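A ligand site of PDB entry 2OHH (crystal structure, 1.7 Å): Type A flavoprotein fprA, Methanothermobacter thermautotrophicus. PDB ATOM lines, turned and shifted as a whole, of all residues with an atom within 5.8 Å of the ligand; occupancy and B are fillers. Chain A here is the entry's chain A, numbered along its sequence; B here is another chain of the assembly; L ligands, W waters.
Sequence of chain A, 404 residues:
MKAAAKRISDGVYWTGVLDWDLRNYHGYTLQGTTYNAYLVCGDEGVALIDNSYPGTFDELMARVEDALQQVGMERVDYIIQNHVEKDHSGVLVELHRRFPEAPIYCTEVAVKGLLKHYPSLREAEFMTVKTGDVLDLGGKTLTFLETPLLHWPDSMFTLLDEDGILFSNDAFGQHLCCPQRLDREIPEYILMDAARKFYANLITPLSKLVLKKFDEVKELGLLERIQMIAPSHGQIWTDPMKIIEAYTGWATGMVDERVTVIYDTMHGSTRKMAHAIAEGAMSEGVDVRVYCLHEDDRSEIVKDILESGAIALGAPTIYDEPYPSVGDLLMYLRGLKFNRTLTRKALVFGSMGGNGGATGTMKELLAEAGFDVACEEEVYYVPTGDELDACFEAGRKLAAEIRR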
ATOM      1  N   ASP A 264      -5.567  -2.894 -13.010  1.00  0.00           N
ATOM      2  CA  ASP A 264      -4.438  -3.824 -13.171  1.00  0.00           C
ATOM      3  C   ASP A 264      -3.763  -3.856 -11.832  1.00  0.00           C
ATOM      4  O   ASP A 264      -4.058  -3.047 -10.957  1.00  0.00           O
ATOM      5  CB  ASP A 264      -3.450  -3.399 -14.258  1.00  0.00           C
ATOM      6  CG  ASP A 264      -2.832  -4.569 -14.986  1.00  0.00           C
ATOM      7  OD1 ASP A 264      -2.804  -5.661 -14.383  1.00  0.00           O
ATOM      8  OD2 ASP A 264      -2.489  -4.441 -16.187  1.00  0.00           O
ATOM      9  N   THR A 265      -2.858  -4.806 -11.713  1.00  0.00           N
ATOM     10  CA  THR A 265      -2.211  -5.070 -10.452  1.00  0.00           C
ATOM     11  C   THR A 265      -0.952  -5.857 -10.774  1.00  0.00           C
ATOM     12  O   THR A 265      -0.821  -6.553 -11.807  1.00  0.00           O
ATOM     13  CB  THR A 265      -3.171  -5.843  -9.585  1.00  0.00           C
ATOM     14  OG1 THR A 265      -2.731  -5.911  -8.219  1.00  0.00           O
ATOM     15  CG2 THR A 265      -3.384  -7.228 -10.108  1.00  0.00           C
ATOM     16  N   MET A 266      -0.015  -5.739  -9.844  1.00  0.00           N
ATOM     17  CA  MET A 266       1.243  -6.432  -9.951  1.00  0.00           C
ATOM     18  C   MET A 266       1.213  -7.518  -8.910  1.00  0.00           C
ATOM     19  O   MET A 266       1.563  -8.665  -9.188  1.00  0.00           O
ATOM     20  CB  MET A 266       2.358  -5.434  -9.703  1.00  0.00           C
ATOM     21  CG  MET A 266       2.618  -4.528 -10.859  1.00  0.00           C
ATOM     22  SD  MET A 266       3.935  -3.371 -10.549  1.00  0.00           S
ATOM     23  CE  MET A 266       3.328  -2.352  -9.201  1.00  0.00           C
ATOM     24  N   HIS A 267       0.784  -7.144  -7.707  1.00  0.00           N
ATOM     25  CA  HIS A 267       0.841  -7.981  -6.528  1.00  0.00           C
ATOM     26  C   HIS A 267      -0.531  -8.352  -5.990  1.00  0.00           C
ATOM     27  O   HIS A 267      -0.629  -9.095  -5.014  1.00  0.00           O
ATOM     28  CB  HIS A 267       1.709  -7.331  -5.451  1.00  0.00           C
ATOM     29  CG  HIS A 267       3.155  -7.282  -5.820  1.00  0.00           C
ATOM     30  ND1 HIS A 267       3.967  -6.194  -5.573  1.00  0.00           N
ATOM     31  CD2 HIS A 267       3.942  -8.200  -6.423  1.00  0.00           C
ATOM     32  CE1 HIS A 267       5.179  -6.444  -6.019  1.00  0.00           C
ATOM     33  NE2 HIS A 267       5.200  -7.670  -6.522  1.00  0.00           N
ATOM     34  N   GLY A 268      -1.597  -7.861  -6.617  1.00  0.00           N
ATOM     35  CA  GLY A 268      -2.943  -8.243  -6.244  1.00  0.00           C
ATOM     36  C   GLY A 268      -3.755  -7.342  -5.307  1.00  0.00           C
ATOM     37  O   GLY A 268      -4.949  -7.569  -5.120  1.00  0.00           O
ATOM     38  N   SER A 269      -3.124  -6.317  -4.731  1.00  0.00           N
ATOM     39  CA  SER A 269      -3.847  -5.446  -3.814  1.00  0.00           C
ATOM     40  C   SER A 269      -4.858  -4.629  -4.550  1.00  0.00           C
ATOM     41  O   SER A 269      -5.987  -4.450  -4.091  1.00  0.00           O
ATOM     42  CB  SER A 269      -2.882  -4.545  -3.081  1.00  0.00           C
ATOM     43  OG  SER A 269      -2.138  -5.361  -2.196  1.00  0.00           O
ATOM     44  N   THR A 270      -4.474  -4.137  -5.724  1.00  0.00           N
ATOM     45  CA  THR A 270      -5.437  -3.358  -6.501  1.00  0.00           C
ATOM     46  C   THR A 270      -6.600  -4.222  -6.976  1.00  0.00           C
ATOM     47  O   THR A 270      -7.740  -3.760  -7.084  1.00  0.00           O
ATOM     48  CB  THR A 270      -4.739  -2.628  -7.683  1.00  0.00           C
ATOM     49  OG1 THR A 270      -3.713  -1.794  -7.121  1.00  0.00           O
ATOM     50  CG2 THR A 270      -5.734  -1.741  -8.423  1.00  0.00           C
ATOM     51  N   ARG A 271      -6.310  -5.488  -7.281  1.00  0.00           N
ATOM     52  CA  ARG A 271      -7.380  -6.440  -7.533  1.00  0.00           C
ATOM     53  C   ARG A 271      -8.332  -6.634  -6.310  1.00  0.00           C
ATOM     54  O   ARG A 271      -9.526  -6.677  -6.458  1.00  0.00           O
ATOM     55  CB  ARG A 271      -6.780  -7.793  -7.962  1.00  0.00           C
ATOM     56  CG  ARG A 271      -7.850  -8.842  -8.188  1.00  0.00           C
ATOM     57  CD  ARG A 271      -7.241 -10.051  -8.789  1.00  0.00           C
ATOM     58  NE  ARG A 271      -6.450 -10.738  -7.791  1.00  0.00           N
ATOM     59  CZ  ARG A 271      -5.140 -10.960  -7.877  1.00  0.00           C
ATOM     60  NH1 ARG A 271      -4.445 -10.555  -8.956  1.00  0.00           N
ATOM     61  NH2 ARG A 271      -4.536 -11.608  -6.885  1.00  0.00           N
ATOM     62  N   ALA A 315      -5.040   0.987 -10.497  1.00  0.00           N
ATOM     63  CA  ALA A 315      -3.692   0.508 -10.842  1.00  0.00           C
ATOM     64  C   ALA A 315      -2.740   0.884  -9.740  1.00  0.00           C
ATOM     65  O   ALA A 315      -2.877   1.975  -9.151  1.00  0.00           O
ATOM     66  CB  ALA A 315      -3.218   1.165 -12.132  1.00  0.00           C
ATOM     67  N   PRO A 316      -1.751   0.031  -9.500  1.00  0.00           N
ATOM     68  CA  PRO A 316      -0.687   0.336  -8.568  1.00  0.00           C
ATOM     69  C   PRO A 316       0.235   1.403  -9.097  1.00  0.00           C
ATOM     70  O   PRO A 316       0.233   1.723 -10.290  1.00  0.00           O
ATOM     71  CB  PRO A 316       0.066  -0.976  -8.486  1.00  0.00           C
ATOM     72  CG  PRO A 316      -0.174  -1.684  -9.815  1.00  0.00           C
ATOM     73  CD  PRO A 316      -1.604  -1.294 -10.107  1.00  0.00           C
ATOM     74  N   THR A 317       1.081   1.938  -8.238  1.00  0.00           N
ATOM     75  CA  THR A 317       2.043   2.916  -8.698  1.00  0.00           C
ATOM     76  C   THR A 317       3.365   2.203  -8.937  1.00  0.00           C
ATOM     77  O   THR A 317       3.760   1.390  -8.117  1.00  0.00           O
ATOM     78  CB  THR A 317       2.278   3.993  -7.667  1.00  0.00           C
ATOM     79  OG1 THR A 317       1.066   4.706  -7.441  1.00  0.00           O
ATOM     80  CG2 THR A 317       3.312   4.976  -8.164  1.00  0.00           C
ATOM     81  N   ILE A 318       3.982   2.505 -10.071  1.00  0.00           N
ATOM     82  CA  ILE A 318       5.297   1.989 -10.429  1.00  0.00           C
ATOM     83  C   ILE A 318       6.136   3.211 -10.796  1.00  0.00           C
ATOM     84  O   ILE A 318       5.839   3.937 -11.737  1.00  0.00           O
ATOM     85  CB  ILE A 318       5.255   0.892 -11.546  1.00  0.00           C
ATOM     86  CG1 ILE A 318       6.642   0.625 -12.125  1.00  0.00           C
ATOM     87  CG2 ILE A 318       4.291   1.281 -12.650  1.00  0.00           C
ATOM     88  CD1 ILE A 318       6.856  -0.853 -12.754  1.00  0.00           C
ATOM     89  N   TYR A 319       7.182   3.480 -10.001  1.00  0.00           N
ATOM     90  CA  TYR A 319       8.041   4.631 -10.268  1.00  0.00           C
ATOM     91  C   TYR A 319       7.264   5.897 -10.587  1.00  0.00           C
ATOM     92  O   TYR A 319       7.474   6.531 -11.626  1.00  0.00           O
ATOM     93  CB  TYR A 319       9.072   4.322 -11.331  1.00  0.00           C
ATOM     94  CG  TYR A 319       9.936   3.162 -10.944  1.00  0.00           C
ATOM     95  CD1 TYR A 319      10.470   3.100  -9.658  1.00  0.00           C
ATOM     96  CD2 TYR A 319      10.234   2.147 -11.844  1.00  0.00           C
ATOM     97  CE1 TYR A 319      11.265   2.063  -9.276  1.00  0.00           C
ATOM     98  CE2 TYR A 319      11.057   1.088 -11.449  1.00  0.00           C
ATOM     99  CZ  TYR A 319      11.554   1.057 -10.172  1.00  0.00           C
ATOM    100  OH  TYR A 319      12.398   0.035  -9.742  1.00  0.00           O
ATOM    101  N   ASP A 320       6.412   6.252  -9.642  1.00  0.00           N
ATOM    102  CA  ASP A 320       5.553   7.432  -9.624  1.00  0.00           C
ATOM    103  C   ASP A 320       4.436   7.398 -10.638  1.00  0.00           C
ATOM    104  O   ASP A 320       3.618   8.324 -10.705  1.00  0.00           O
ATOM    105  CB  ASP A 320       6.309   8.780  -9.661  1.00  0.00           C
ATOM    106  CG  ASP A 320       7.452   8.856  -8.702  1.00  0.00           C
ATOM    107  OD1 ASP A 320       7.304   8.420  -7.532  1.00  0.00           O
ATOM    108  OD2 ASP A 320       8.493   9.409  -9.098  1.00  0.00           O
ATOM    109  N   GLU A 321       4.352   6.320 -11.425  1.00  0.00           N
ATOM    110  CA  GLU A 321       3.350   6.326 -12.462  1.00  0.00           C
ATOM    111  C   GLU A 321       2.368   5.213 -12.266  1.00  0.00           C
ATOM    112  O   GLU A 321       2.636   4.299 -11.516  1.00  0.00           O
ATOM    113  CB  GLU A 321       3.962   6.119 -13.854  1.00  0.00           C
ATOM    114  CG  GLU A 321       5.007   7.150 -14.276  1.00  0.00           C
ATOM    115  CD  GLU A 321       4.450   8.510 -14.601  1.00  0.00           C
ATOM    116  OE1 GLU A 321       3.245   8.626 -14.866  1.00  0.00           O
ATOM    117  OE2 GLU A 321       5.240   9.462 -14.618  1.00  0.00           O
ATOM    118  N   SER A 351      -3.294   0.532  -5.150  1.00  0.00           N
ATOM    119  CA  SER A 351      -2.411   0.352  -4.038  1.00  0.00           C
ATOM    120  C   SER A 351      -1.089   1.039  -4.377  1.00  0.00           C
ATOM    121  O   SER A 351      -0.731   1.240  -5.546  1.00  0.00           O
ATOM    122  CB  SER A 351      -2.193  -1.139  -3.807  1.00  0.00           C
ATOM    123  OG  SER A 351      -1.390  -1.291  -2.675  1.00  0.00           O
ATOM    124  N   MET A 352      -0.336   1.392  -3.353  1.00  0.00           N
ATOM    125  CA  MET A 352       0.979   1.912  -3.661  1.00  0.00           C
ATOM    126  C   MET A 352       1.868   1.618  -2.475  1.00  0.00           C
ATOM    127  O   MET A 352       1.378   1.101  -1.465  1.00  0.00           O
ATOM    128  CB  MET A 352       0.896   3.400  -3.985  1.00  0.00           C
ATOM    129  CG  MET A 352       0.021   4.174  -3.022  1.00  0.00           C
ATOM    130  SD  MET A 352       0.972   4.587  -1.564  1.00  0.00           S
ATOM    131  CE  MET A 352      -0.321   5.314  -0.552  1.00  0.00           C
ATOM    132  N   GLY A 353       3.150   1.958  -2.589  1.00  0.00           N
ATOM    133  CA  GLY A 353       4.102   1.495  -1.598  1.00  0.00           C
ATOM    134  C   GLY A 353       4.911   2.608  -1.013  1.00  0.00           C
ATOM    135  O   GLY A 353       5.789   2.375  -0.151  1.00  0.00           O
ATOM    136  N   GLY A 354       4.649   3.833  -1.480  1.00  0.00           N
ATOM    137  CA  GLY A 354       5.562   4.938  -1.214  1.00  0.00           C
ATOM    138  C   GLY A 354       4.769   6.205  -1.394  1.00  0.00           C
ATOM    139  O   GLY A 354       3.754   6.407  -0.726  1.00  0.00           O
ATOM    140  N   ASN A 355       5.214   7.037  -2.322  1.00  0.00           N
ATOM    141  CA  ASN A 355       4.523   8.294  -2.557  1.00  0.00           C
ATOM    142  C   ASN A 355       3.258   8.133  -3.414  1.00  0.00           C
ATOM    143  O   ASN A 355       2.516   9.076  -3.579  1.00  0.00           O
ATOM    144  CB  ASN A 355       5.474   9.298  -3.200  1.00  0.00           C
ATOM    145  CG  ASN A 355       6.580   9.730  -2.272  1.00  0.00           C
ATOM    146  OD1 ASN A 355       7.713   9.957  -2.695  1.00  0.00           O
ATOM    147  ND2 ASN A 355       6.257   9.861  -1.002  1.00  0.00           N
ATOM    148  N   GLY A 356       3.003   6.956  -3.950  1.00  0.00           N
ATOM    149  CA  GLY A 356       1.875   6.844  -4.847  1.00  0.00           C
ATOM    150  C   GLY A 356       2.035   7.731  -6.059  1.00  0.00           C
ATOM    151  O   GLY A 356       3.133   8.151  -6.410  1.00  0.00           O
ATOM    152  N   GLY A 357       0.924   8.050  -6.684  1.00  0.00           N
ATOM    153  CA  GLY A 357       0.988   8.893  -7.849  1.00  0.00           C
ATOM    154  C   GLY A 357       0.145   8.287  -8.945  1.00  0.00           C
ATOM    155  O   GLY A 357      -0.296   9.021  -9.803  1.00  0.00           O
ATOM    156  N   VAL A 379      -4.551   2.971  -1.281  1.00  0.00           N
ATOM    157  CA  VAL A 379      -4.235   2.081  -0.178  1.00  0.00           C
ATOM    158  C   VAL A 379      -2.748   1.847  -0.184  1.00  0.00           C
ATOM    159  O   VAL A 379      -2.137   1.790  -1.235  1.00  0.00           O
ATOM    160  CB  VAL A 379      -5.074   0.773  -0.242  1.00  0.00           C
ATOM    161  CG1 VAL A 379      -4.492  -0.305   0.595  1.00  0.00           C
ATOM    162  CG2 VAL A 379      -6.503   1.079   0.252  1.00  0.00           C
ATOM    163  N   TYR A 380      -2.157   1.818   0.998  1.00  0.00           N
ATOM    164  CA  TYR A 380      -0.750   1.532   1.093  1.00  0.00           C
ATOM    165  C   TYR A 380      -0.646   0.019   1.115  1.00  0.00           C
ATOM    166  O   TYR A 380      -1.154  -0.626   2.028  1.00  0.00           O
ATOM    167  CB  TYR A 380      -0.288   2.132   2.404  1.00  0.00           C
ATOM    168  CG  TYR A 380       1.131   1.873   2.769  1.00  0.00           C
ATOM    169  CD1 TYR A 380       2.184   2.237   1.920  1.00  0.00           C
ATOM    170  CD2 TYR A 380       1.420   1.293   3.978  1.00  0.00           C
ATOM    171  CE1 TYR A 380       3.496   2.028   2.292  1.00  0.00           C
ATOM    172  CE2 TYR A 380       2.721   1.071   4.354  1.00  0.00           C
ATOM    173  CZ  TYR A 380       3.754   1.441   3.517  1.00  0.00           C
ATOM    174  OH  TYR A 380       5.033   1.214   3.923  1.00  0.00           O
ATOM    175  N   TYR A 381      -0.010  -0.541   0.091  1.00  0.00           N
ATOM    176  CA  TYR A 381       0.186  -1.978  -0.008  1.00  0.00           C
ATOM    177  C   TYR A 381      -1.142  -2.727   0.098  1.00  0.00           C
ATOM    178  O   TYR A 381      -2.080  -2.446  -0.661  1.00  0.00           O
ATOM    179  CB  TYR A 381       1.207  -2.448   1.008  1.00  0.00           C
ATOM    180  CG  TYR A 381       2.617  -2.011   0.673  1.00  0.00           C
ATOM    181  CD1 TYR A 381       3.149  -2.261  -0.577  1.00  0.00           C
ATOM    182  CD2 TYR A 381       3.400  -1.363   1.602  1.00  0.00           C
ATOM    183  CE1 TYR A 381       4.460  -1.894  -0.880  1.00  0.00           C
ATOM    184  CE2 TYR A 381       4.703  -0.986   1.303  1.00  0.00           C
ATOM    185  CZ  TYR A 381       5.214  -1.243   0.048  1.00  0.00           C
ATOM    186  OH  TYR A 381       6.506  -0.870  -0.243  1.00  0.00           O
ATOM    187  N   VAL A 382      -1.225  -3.654   1.051  1.00  0.00           N
ATOM    188  CA  VAL A 382      -2.346  -4.573   1.126  1.00  0.00           C
ATOM    189  C   VAL A 382      -3.465  -3.928   1.899  1.00  0.00           C
ATOM    190  O   VAL A 382      -3.242  -3.498   3.010  1.00  0.00           O
ATOM    191  CB  VAL A 382      -1.970  -5.884   1.809  1.00  0.00           C
ATOM    192  CG1 VAL A 382      -3.210  -6.779   1.898  1.00  0.00           C
ATOM    193  CG2 VAL A 382      -0.846  -6.596   1.032  1.00  0.00           C
ATOM    194  N   HIS B  26       5.104  -8.203 -12.871  1.00  0.00           N
ATOM    195  CA  HIS B  26       4.840  -6.781 -12.879  1.00  0.00           C
ATOM    196  C   HIS B  26       5.246  -6.125 -14.199  1.00  0.00           C
ATOM    197  O   HIS B  26       6.002  -5.125 -14.273  1.00  0.00           O
ATOM    198  CB  HIS B  26       5.413  -6.093 -11.634  1.00  0.00           C
ATOM    199  CG  HIS B  26       6.898  -6.076 -11.532  1.00  0.00           C
ATOM    200  ND1 HIS B  26       7.716  -5.593 -12.520  1.00  0.00           N
ATOM    201  CD2 HIS B  26       7.720  -6.404 -10.499  1.00  0.00           C
ATOM    202  CE1 HIS B  26       8.979  -5.677 -12.139  1.00  0.00           C
ATOM    203  NE2 HIS B  26       9.004  -6.163 -10.901  1.00  0.00           N
ATOM    204  N   GLU B  85       9.100  -6.222  -0.510  1.00  0.00           N
ATOM    205  CA  GLU B  85       8.296  -6.744  -1.635  1.00  0.00           C
ATOM    206  C   GLU B  85       8.033  -8.227  -1.422  1.00  0.00           C
ATOM    207  O   GLU B  85       8.903  -8.948  -0.956  1.00  0.00           O
ATOM    208  CB  GLU B  85       8.996  -6.504  -2.970  1.00  0.00           C
ATOM    209  CG  GLU B  85       8.114  -6.715  -4.225  1.00  0.00           C
ATOM    210  CD  GLU B  85       8.778  -6.196  -5.519  1.00  0.00           C
ATOM    211  OE1 GLU B  85       9.821  -5.509  -5.445  1.00  0.00           O
ATOM    212  OE2 GLU B  85       8.238  -6.451  -6.616  1.00  0.00           O
ATOM    213  N   HIS B 117       1.774  -5.520   4.874  1.00  0.00           N
ATOM    214  CA  HIS B 117       1.570  -6.769   4.175  1.00  0.00           C
ATOM    215  C   HIS B 117       1.121  -7.890   5.064  1.00  0.00           C
ATOM    216  O   HIS B 117       0.280  -8.702   4.683  1.00  0.00           O
ATOM    217  CB  HIS B 117       2.856  -7.209   3.488  1.00  0.00           C
ATOM    218  CG  HIS B 117       3.190  -6.408   2.267  1.00  0.00           C
ATOM    219  ND1 HIS B 117       3.790  -5.178   2.333  1.00  0.00           N
ATOM    220  CD2 HIS B 117       2.999  -6.676   0.951  1.00  0.00           C
ATOM    221  CE1 HIS B 117       3.982  -4.725   1.107  1.00  0.00           C
ATOM    222  NE2 HIS B 117       3.506  -5.612   0.255  1.00  0.00           N
ATOM    223  N   HIS B 151      15.387  -0.833  -4.701  1.00  0.00           N
ATOM    224  CA  HIS B 151      14.542  -0.006  -5.554  1.00  0.00           C
ATOM    225  C   HIS B 151      13.345   0.636  -4.847  1.00  0.00           C
ATOM    226  O   HIS B 151      12.617   1.417  -5.474  1.00  0.00           O
ATOM    227  CB  HIS B 151      14.094  -0.771  -6.820  1.00  0.00           C
ATOM    228  CG  HIS B 151      13.109  -1.875  -6.561  1.00  0.00           C
ATOM    229  ND1 HIS B 151      11.980  -2.052  -7.346  1.00  0.00           N
ATOM    230  CD2 HIS B 151      13.093  -2.860  -5.635  1.00  0.00           C
ATOM    231  CE1 HIS B 151      11.314  -3.109  -6.903  1.00  0.00           C
ATOM    232  NE2 HIS B 151      11.969  -3.620  -5.874  1.00  0.00           N
ATOM    233  N   TRP B 152      13.174   0.339  -3.554  1.00  0.00           N
ATOM    234  CA  TRP B 152      12.051   0.844  -2.779  1.00  0.00           C
ATOM    235  C   TRP B 152      12.538   1.673  -1.566  1.00  0.00           C
ATOM    236  O   TRP B 152      13.692   1.527  -1.126  1.00  0.00           O
ATOM    237  CB  TRP B 152      11.171  -0.332  -2.286  1.00  0.00           C
ATOM    238  CG  TRP B 152      10.185  -0.931  -3.299  1.00  0.00           C
ATOM    239  CD1 TRP B 152      10.195  -0.777  -4.666  1.00  0.00           C
ATOM    240  CD2 TRP B 152       9.078  -1.818  -3.019  1.00  0.00           C
ATOM    241  NE1 TRP B 152       9.151  -1.470  -5.229  1.00  0.00           N
ATOM    242  CE2 TRP B 152       8.458  -2.130  -4.250  1.00  0.00           C
ATOM    243  CE3 TRP B 152       8.547  -2.374  -1.838  1.00  0.00           C
ATOM    244  CZ2 TRP B 152       7.341  -2.975  -4.341  1.00  0.00           C
ATOM    245  CZ3 TRP B 152       7.430  -3.211  -1.924  1.00  0.00           C
ATOM    246  CH2 TRP B 152       6.843  -3.493  -3.169  1.00  0.00           C
ATOM    247  N   ASN B 201      14.641  -2.050 -16.714  1.00  0.00           N
ATOM    248  CA  ASN B 201      13.238  -2.018 -16.249  1.00  0.00           C
ATOM    249  C   ASN B 201      13.067  -1.581 -14.824  1.00  0.00           C
ATOM    250  O   ASN B 201      11.996  -1.121 -14.417  1.00  0.00           O
ATOM    251  CB  ASN B 201      12.638  -3.403 -16.427  1.00  0.00           C
ATOM    252  CG  ASN B 201      12.271  -3.660 -17.822  1.00  0.00           C
ATOM    253  OD1 ASN B 201      11.219  -3.266 -18.261  1.00  0.00           O
ATOM    254  ND2 ASN B 201      13.171  -4.273 -18.563  1.00  0.00           N
ATOM    255  N   LEU B 202      14.101  -1.779 -14.020  1.00  0.00           N
ATOM    256  CA  LEU B 202      13.941  -1.567 -12.608  1.00  0.00           C
ATOM    257  C   LEU B 202      14.880  -0.510 -12.123  1.00  0.00           C
ATOM    258  O   LEU B 202      14.615   0.132 -11.121  1.00  0.00           O
ATOM    259  CB  LEU B 202      14.184  -2.883 -11.882  1.00  0.00           C
ATOM    260  CG  LEU B 202      13.101  -3.910 -12.223  1.00  0.00           C
ATOM    261  CD1 LEU B 202      13.542  -5.311 -11.852  1.00  0.00           C
ATOM    262  CD2 LEU B 202      11.799  -3.529 -11.514  1.00  0.00           C
HETATM  263  N1  LIG L   1       4.838   2.495  -5.049  1.00  0.00           N
HETATM  264  C1  LIG L   1       4.878   3.879  -4.947  1.00  0.00           C
HETATM  265  O1  LIG L   1       4.117   4.396  -4.132  1.00  0.00           O
HETATM  266  N2  LIG L   1       5.750   4.614  -5.717  1.00  0.00           N
HETATM  267  C2  LIG L   1       6.608   4.019  -6.625  1.00  0.00           C
HETATM  268  O2  LIG L   1       7.303   4.712  -7.343  1.00  0.00           O
HETATM  269  C3  LIG L   1       6.588   2.629  -6.740  1.00  0.00           C
HETATM  270  N3  LIG L   1       7.441   1.979  -7.634  1.00  0.00           N
HETATM  271  C4  LIG L   1       7.342   0.604  -7.748  1.00  0.00           C
HETATM  272  C5  LIG L   1       8.167  -0.024  -8.655  1.00  0.00           C
HETATM  273  C6  LIG L   1       8.129  -1.408  -8.780  1.00  0.00           C
HETATM  274  C7  LIG L   1       8.996  -1.988  -9.876  1.00  0.00           C
HETATM  275  C8  LIG L   1       7.234  -2.159  -7.999  1.00  0.00           C
HETATM  276  C9  LIG L   1       6.830  -3.517  -8.467  1.00  0.00           C
HETATM  277  C10 LIG L   1       6.391  -1.515  -7.096  1.00  0.00           C
HETATM  278  C11 LIG L   1       6.440  -0.120  -6.952  1.00  0.00           C
HETATM  279  N4  LIG L   1       5.607   0.540  -6.039  1.00  0.00           N
HETATM  280  C12 LIG L   1       5.705   1.897  -5.935  1.00  0.00           C
HETATM  281  C13 LIG L   1       5.012  -0.184  -4.879  1.00  0.00           C
HETATM  282  C14 LIG L   1       3.662  -0.742  -5.301  1.00  0.00           C
HETATM  283  O3  LIG L   1       2.887   0.350  -5.800  1.00  0.00           O
HETATM  284  C15 LIG L   1       3.035  -1.474  -4.125  1.00  0.00           C
HETATM  285  O4  LIG L   1       3.672  -2.755  -4.082  1.00  0.00           O
HETATM  286  C16 LIG L   1       1.539  -1.668  -4.318  1.00  0.00           C
HETATM  287  O5  LIG L   1       0.942  -2.321  -3.221  1.00  0.00           O
HETATM  288  C17 LIG L   1       1.296  -2.650  -5.434  1.00  0.00           C
HETATM  289  O6  LIG L   1      -0.109  -2.745  -5.689  1.00  0.00           O
HETATM  290  P1  LIG L   1      -0.680  -4.063  -6.426  1.00  0.00           P
HETATM  291  O7  LIG L   1      -0.711  -5.182  -5.429  1.00  0.00           O
HETATM  292  O8  LIG L   1      -2.101  -3.926  -7.001  1.00  0.00           O
HETATM  293  O9  LIG L   1       0.255  -4.359  -7.561  1.00  0.00           O
HETATM  294  O   HOH W   1       8.055   3.392  -3.867  1.00  0.00           O
HETATM  295  O   HOH W   2       9.518   2.572  -6.257  1.00  0.00           O
HETATM  296  O   HOH W   3       7.667   5.779  -3.369  1.00  0.00           O
HETATM  297  O   HOH W   4       0.482  -4.827  -3.138  1.00  0.00           O
HETATM  298  O   HOH W   5       5.616   7.016  -5.753  1.00  0.00           O
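OG1 of Thr 270 lies within hydrogen-bond range of O8 of the ligand (2.7 Å). An oxygen (O2) of the ligand is in hydrogen-bond range of the backbone NH (N) of Asp 320, 2.9 Å away. O5 of the ligand sits at hydrogen-bond distance from OG of Ser 351, 2.6 Å away. An oxygen (O1) of the ligand sits at hydrogen-bond distance from the backbone NH (N) of Asn 355 (3.4 Å). The backbone NH of Thr 270 sits at hydrogen-bond distance from an oxygen (O8) of the ligand (2.7 Å). O7 of the ligand lies within hydrogen-bond range of N of Ser 269 (2.8 Å). An oxygen (O3) of the ligand sits at hydrogen-bond distance from the backbone NH of Thr 317 (3.4 Å). O of Thr 317 lies within hydrogen-bond range of O3 of the ligand (2.7 Å). N of Tyr 319 is in hydrogen-bond range of N3 of the ligand. The side-chain hydroxyl of Thr 265 is in hydrogen-bond range of an oxygen (O8) of the ligand, 2.4 Å away. O9 of the ligand lies within hydrogen-bond range of N of Met 266 (2.7 Å). The backbone NH (N) of Gly 354 lies within hydrogen-bond range of an oxygen (O1) of the ligand (2.8 Å). A nitrogen (N1) of the ligand sits at hydrogen-bond distance from the backbone NH (N) of Gly 353. N of Gly 268 sits at hydrogen-bond distance from O7 of the ligand (3.1 Å). An oxygen (O9) of the ligand sits at hydrogen-bond distance from the backbone NH (N) of His 267. N of Gly 356 is in hydrogen-bond range of O1 of the ligand, 2.8 Å away.
Pro 316 touches the ligand (CB to O6, 3.3 Å). Ile 318 touches the ligand. Met 352 touches the ligand. CA of Tyr 381 touches O5 of the ligand (3.3 Å). His 26 of chain B touches the ligand (CD2 to C9, 3.6 Å). Glu 85 of chain B touches the ligand. His 151 of chain B touches the ligand. Trp 152 of chain B touches the ligand. CD2 of Leu 202 of chain B touches C7 of the ligand, at 3.6 Å. Hydrophobic or aromatic side chains that line the ligand: Met 266, His 267, Pro 316, Ile 318, Tyr 319, Met 352, Tyr 381, His 26 of chain B, His 151 of chain B, Trp 152 of chain B and Leu 202 of chain B. The nearest printed residue that does not touch the ligand is Arg 271 (4.5 Å).
Water W5 lies within hydrogen-bond range of N2 of the ligand (2.4 Å), O of Gly 356 (2.8 Å), OD1 of Asp 320 (2.8 Å) and N of Asn 355 (3.5 Å). Water W4 lies within hydrogen-bond range of an oxygen (O5) of the ligand and the side-chain hydroxyl of Ser 269. Water W2 bridges a nitrogen (N3) of the ligand (2.6 Å) and the backbone carbonyl oxygen (O) of His 151 of chain B (3.4 Å). Water W3 bridges the backbone NH (N) of Asn 355 (2.9 Å) and a nitrogen (N2) of the ligand (3.2 Å).
O of Met 352 is in hydrogen-bond range of N of Tyr 381 (2.7 Å). The side-chain hydroxyl of Ser 269 lies within hydrogen-bond range of the backbone carbonyl oxygen of Tyr 381, at 3.3 Å. OG1 of Thr 317 sits at hydrogen-bond distance from N of Gly 357, at 3.4 Å. The side-chain hydroxyl (OG1) of Thr 265 is in hydrogen-bond range of the backbone NH (N) of Gly 268, at 2.8 Å. The side-chain hydroxyl of Ser 351 lies close to the backbone carbonyl oxygen of Val 379 (3.5 Å). The backbone NH of Gly 354 lies close to the side-chain sulfur of Met 352 (3.8 Å). The backbone carbonyl oxygen of Gly 353 lies within hydrogen-bond range of the side-chain hydroxyl of Tyr 381 (3.3 Å). The side-chain hydroxyl (OG) of Ser 351 is in hydrogen-bond range of the backbone carbonyl oxygen (O) of Tyr 381 (2.4 Å).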
